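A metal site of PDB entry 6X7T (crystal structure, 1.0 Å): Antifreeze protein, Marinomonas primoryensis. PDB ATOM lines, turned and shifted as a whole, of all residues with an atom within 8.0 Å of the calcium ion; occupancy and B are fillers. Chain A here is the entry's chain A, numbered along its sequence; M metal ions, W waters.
The side-chain amide nitrogen of Gln 26 lies close to the side-chain amide nitrogen of Asn 127. NE2 of Gln 26 lies within hydrogen-bond range of OD1 of Asn 28, at 2.9 Å. OD2 of Asp 110 lies close to N of Gln 155. The side-chain carboxylate (OD1) of Asp 86 lies close to the side-chain hydroxyl (OG1) of Thr 85 (2.7 Å). The side-chain carboxylate (OD2) of Asp 86 lies close to the backbone NH (N) of Leu 27. The backbone carbonyl oxygen of Asp 86 lies within hydrogen-bond range of the backbone NH of Thr 23 (2.9 Å).
Of the 18 residues printed, 3 come within 4 Å of the calcium ion.
The calcium ion is bound by the side-chain amide oxygen (OE1) of Gln 26 (2.3 Å), the backbone carbonyl oxygen (O) of Gln 155 (2.3 Å), water W1 (2.4 Å), water W2 (2.4 Å), the side-chain carboxylate (OD1) of Asp 86 (2.4 Å), water W3 (2.4 Å) and the side-chain carboxylate (OD2) of Asp 86 (2.5 Å).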
ATOM      1  N   THR A  23      23.278  14.091  13.377  1.00  0.00           N
ATOM      2  CA  THR A  23      23.843  14.197  14.712  1.00  0.00           C
ATOM      3  C   THR A  23      22.917  13.517  15.708  1.00  0.00           C
ATOM      4  O   THR A  23      21.727  13.350  15.449  1.00  0.00           O
ATOM      5  CB  THR A  23      24.082  15.670  15.104  1.00  0.00           C
ATOM      6  OG1 THR A  23      24.750  15.753  16.360  1.00  0.00           O
ATOM      7  CG2 THR A  23      22.784  16.486  15.239  1.00  0.00           C
ATOM      8  N   ASN A  24      23.459  13.172  16.877  1.00  0.00           N
ATOM      9  CA  ASN A  24      22.662  12.642  17.979  1.00  0.00           C
ATOM     10  C   ASN A  24      22.492  13.656  19.108  1.00  0.00           C
ATOM     11  O   ASN A  24      22.015  13.299  20.191  1.00  0.00           O
ATOM     12  CB  ASN A  24      23.262  11.335  18.481  1.00  0.00           C
ATOM     13  CG  ASN A  24      23.315  10.305  17.373  1.00  0.00           C
ATOM     14  OD1 ASN A  24      22.377  10.182  16.594  1.00  0.00           O
ATOM     15  ND2 ASN A  24      24.436   9.609  17.267  1.00  0.00           N
ATOM     16  N   SER A  25      22.837  14.910  18.857  1.00  0.00           N
ATOM     17  CA  SER A  25      22.501  16.028  19.713  1.00  0.00           C
ATOM     18  C   SER A  25      21.266  16.734  19.168  1.00  0.00           C
ATOM     19  O   SER A  25      20.869  16.544  18.025  1.00  0.00           O
ATOM     20  CB  SER A  25      23.679  16.994  19.819  1.00  0.00           C
ATOM     21  OG  SER A  25      23.957  17.607  18.580  1.00  0.00           O
ATOM     22  N   GLN A  26      20.663  17.577  20.025  1.00  0.00           N
ATOM     23  CA  GLN A  26      19.430  18.255  19.646  1.00  0.00           C
ATOM     24  C   GLN A  26      19.713  19.478  18.781  1.00  0.00           C
ATOM     25  O   GLN A  26      20.549  20.326  19.125  1.00  0.00           O
ATOM     26  CB  GLN A  26      18.662  18.680  20.901  1.00  0.00           C
ATOM     27  CG  GLN A  26      17.510  19.640  20.648  1.00  0.00           C
ATOM     28  CD  GLN A  26      16.306  19.027  19.925  1.00  0.00           C
ATOM     29  OE1 GLN A  26      16.383  17.930  19.369  1.00  0.00           O
ATOM     30  NE2 GLN A  26      15.202  19.744  19.906  1.00  0.00           N
ATOM     31  N   LEU A  27      18.971  19.602  17.684  1.00  0.00           N
ATOM     32  CA  LEU A  27      18.967  20.814  16.870  1.00  0.00           C
ATOM     33  C   LEU A  27      17.739  21.646  17.244  1.00  0.00           C
ATOM     34  O   LEU A  27      16.612  21.224  17.011  1.00  0.00           O
ATOM     35  CB  LEU A  27      18.923  20.424  15.394  1.00  0.00           C
ATOM     36  CG  LEU A  27      20.124  19.627  14.898  1.00  0.00           C
ATOM     37  CD1 LEU A  27      19.879  19.175  13.456  1.00  0.00           C
ATOM     38  CD2 LEU A  27      21.411  20.417  15.011  1.00  0.00           C
ATOM     39  N   ASN A  28      17.981  22.834  17.825  1.00  0.00           N
ATOM     40  CA  ASN A  28      16.896  23.715  18.239  1.00  0.00           C
ATOM     41  C   ASN A  28      16.742  24.949  17.344  1.00  0.00           C
ATOM     42  O   ASN A  28      15.693  25.593  17.403  1.00  0.00           O
ATOM     43  CB  ASN A  28      17.122  24.213  19.670  1.00  0.00           C
ATOM     44  CG  ASN A  28      16.761  23.171  20.711  1.00  0.00           C
ATOM     45  OD1 ASN A  28      15.713  22.531  20.628  1.00  0.00           O
ATOM     46  ND2 ASN A  28      17.634  22.998  21.691  1.00  0.00           N
ATOM     47  N   ASP A  59      11.569  10.605  11.726  1.00  0.00           N
ATOM     48  CA  ASP A  59      12.918  11.192  11.786  1.00  0.00           C
ATOM     49  C   ASP A  59      13.634  11.156  10.442  1.00  0.00           C
ATOM     50  O   ASP A  59      13.893  10.075   9.890  1.00  0.00           O
ATOM     51  CB  ASP A  59      13.836  10.504  12.819  1.00  0.00           C
ATOM     52  CG  ASP A  59      13.207  10.319  14.175  1.00  0.00           C
ATOM     53  OD1 ASP A  59      12.471  11.201  14.649  1.00  0.00           O
ATOM     54  OD2 ASP A  59      13.490   9.266  14.790  1.00  0.00           O
ATOM     55  N   ASN A  84      20.972   8.636  12.674  1.00  0.00           N
ATOM     56  CA  ASN A  84      21.173   9.698  13.677  1.00  0.00           C
ATOM     57  C   ASN A  84      19.772  10.094  14.161  1.00  0.00           C
ATOM     58  O   ASN A  84      18.758   9.752  13.521  1.00  0.00           O
ATOM     59  CB  ASN A  84      21.886  10.914  13.096  1.00  0.00           C
ATOM     60  CG  ASN A  84      23.405  10.788  13.052  1.00  0.00           C
ATOM     61  OD1 ASN A  84      24.065  10.690  14.111  1.00  0.00           O
ATOM     62  ND2 ASN A  84      23.940  10.830  11.856  1.00  0.00           N
ATOM     63  N   THR A  85      19.703  10.828  15.276  1.00  0.00           N
ATOM     64  CA  THR A  85      18.406  11.286  15.759  1.00  0.00           C
ATOM     65  C   THR A  85      17.930  12.536  15.037  1.00  0.00           C
ATOM     66  O   THR A  85      16.728  12.716  14.824  1.00  0.00           O
ATOM     67  CB  THR A  85      18.428  11.524  17.273  1.00  0.00           C
ATOM     68  OG1 THR A  85      19.300  12.611  17.614  1.00  0.00           O
ATOM     69  CG2 THR A  85      18.886  10.289  18.024  1.00  0.00           C
ATOM     70  N   ASP A  86      18.866  13.412  14.676  1.00  0.00           N
ATOM     71  CA  ASP A  86      18.595  14.741  14.136  1.00  0.00           C
ATOM     72  C   ASP A  86      19.417  14.903  12.866  1.00  0.00           C
ATOM     73  O   ASP A  86      20.496  14.319  12.733  1.00  0.00           O
ATOM     74  CB  ASP A  86      19.025  15.835  15.131  1.00  0.00           C
ATOM     75  CG  ASP A  86      18.149  15.893  16.394  1.00  0.00           C
ATOM     76  OD1 ASP A  86      17.948  14.840  17.050  1.00  0.00           O
ATOM     77  OD2 ASP A  86      17.690  17.001  16.765  1.00  0.00           O
ATOM     78  N   GLY A  87      18.946  15.737  11.932  1.00  0.00           N
ATOM     79  CA  GLY A  87      19.765  15.955  10.751  1.00  0.00           C
ATOM     80  C   GLY A  87      19.225  17.088   9.915  1.00  0.00           C
ATOM     81  O   GLY A  87      18.127  17.568  10.145  1.00  0.00           O
ATOM     82  N   ASP A 110      11.572  21.000  10.306  1.00  0.00           N
ATOM     83  CA  ASP A 110      11.504  22.037  11.330  1.00  0.00           C
ATOM     84  C   ASP A 110      11.809  23.405  10.714  1.00  0.00           C
ATOM     85  O   ASP A 110      11.041  23.857   9.869  1.00  0.00           O
ATOM     86  CB  ASP A 110      12.405  21.614  12.496  1.00  0.00           C
ATOM     87  CG  ASP A 110      11.746  20.542  13.333  1.00  0.00           C
ATOM     88  OD1 ASP A 110      10.868  20.909  14.146  1.00  0.00           O
ATOM     89  OD2 ASP A 110      12.057  19.327  13.140  1.00  0.00           O
ATOM     90  N   ASN A 127      12.153  25.128  16.002  1.00  0.00           N
ATOM     91  CA  ASN A 127      11.448  23.903  15.617  1.00  0.00           C
ATOM     92  C   ASN A 127       9.961  24.155  15.482  1.00  0.00           C
ATOM     93  O   ASN A 127       9.388  25.043  16.133  1.00  0.00           O
ATOM     94  CB  ASN A 127      11.747  22.819  16.649  1.00  0.00           C
ATOM     95  CG  ASN A 127      13.176  22.333  16.546  1.00  0.00           C
ATOM     96  OD1 ASN A 127      13.757  22.328  15.452  1.00  0.00           O
ATOM     97  ND2 ASN A 127      13.770  21.934  17.671  1.00  0.00           N
ATOM     98  N   TRP A 153      16.535  21.852   8.778  1.00  0.00           N
ATOM     99  CA  TRP A 153      16.833  20.695   9.621  1.00  0.00           C
ATOM    100  C   TRP A 153      15.540  20.083  10.161  1.00  0.00           C
ATOM    101  O   TRP A 153      14.461  20.701  10.147  1.00  0.00           O
ATOM    102  CB  TRP A 153      17.815  21.035  10.781  1.00  0.00           C
ATOM    103  CG  TRP A 153      17.130  21.798  11.862  1.00  0.00           C
ATOM    104  CD1 TRP A 153      16.520  21.276  12.980  1.00  0.00           C
ATOM    105  CD2 TRP A 153      16.918  23.217  11.918  1.00  0.00           C
ATOM    106  NE1 TRP A 153      15.934  22.280  13.713  1.00  0.00           N
ATOM    107  CE2 TRP A 153      16.160  23.472  13.086  1.00  0.00           C
ATOM    108  CE3 TRP A 153      17.284  24.289  11.098  1.00  0.00           C
ATOM    109  CZ2 TRP A 153      15.755  24.757  13.449  1.00  0.00           C
ATOM    110  CZ3 TRP A 153      16.889  25.563  11.453  1.00  0.00           C
ATOM    111  CH2 TRP A 153      16.125  25.785  12.621  1.00  0.00           C
ATOM    112  N   ASP A 154      15.708  18.862  10.671  1.00  0.00           N
ATOM    113  CA  ASP A 154      14.707  18.107  11.405  1.00  0.00           C
ATOM    114  C   ASP A 154      15.284  17.749  12.772  1.00  0.00           C
ATOM    115  O   ASP A 154      16.333  17.084  12.867  1.00  0.00           O
ATOM    116  CB  ASP A 154      14.349  16.810  10.660  1.00  0.00           C
ATOM    117  CG  ASP A 154      13.397  15.933  11.455  1.00  0.00           C
ATOM    118  OD1 ASP A 154      12.493  16.506  12.116  1.00  0.00           O
ATOM    119  OD2 ASP A 154      13.547  14.689  11.429  1.00  0.00           O
ATOM    120  N   GLN A 155      14.594  18.176  13.828  1.00  0.00           N
ATOM    121  CA  GLN A 155      14.960  17.787  15.190  1.00  0.00           C
ATOM    122  C   GLN A 155      14.431  16.404  15.566  1.00  0.00           C
ATOM    123  O   GLN A 155      14.777  15.890  16.642  1.00  0.00           O
ATOM    124  CB  GLN A 155      14.419  18.810  16.196  1.00  0.00           C
ATOM    125  CG  GLN A 155      12.910  18.814  16.369  1.00  0.00           C
ATOM    126  CD  GLN A 155      12.446  17.988  17.538  1.00  0.00           C
ATOM    127  OE1 GLN A 155      12.938  18.140  18.669  1.00  0.00           O
ATOM    128  NE2 GLN A 155      11.474  17.115  17.282  1.00  0.00           N
ATOM    129  N   GLY A 156      13.587  15.835  14.709  1.00  0.00           N
ATOM    130  CA  GLY A 156      12.929  14.578  14.981  1.00  0.00           C
ATOM    131  C   GLY A 156      11.466  14.636  14.584  1.00  0.00           C
ATOM    132  O   GLY A 156      10.884  15.723  14.462  1.00  0.00           O
ATOM    133  N   GLY A 157      10.878  13.466  14.389  1.00  0.00           N
ATOM    134  CA  GLY A 157       9.455  13.368  14.087  1.00  0.00           C
ATOM    135  C   GLY A 157       9.185  13.522  12.604  1.00  0.00           C
ATOM    136  O   GLY A 157       9.791  12.836  11.784  1.00  0.00           O
HETATM  137 CA    CA M   1      16.233  15.805  18.456  1.00  0.00          CA
HETATM  138  O   HOH W   1      17.616  15.372  20.320  1.00  0.00           O
HETATM  139  O   HOH W   2      15.512  13.565  18.766  1.00  0.00           O
HETATM  140  O   HOH W   3      14.128  16.013  19.686  1.00  0.00           O
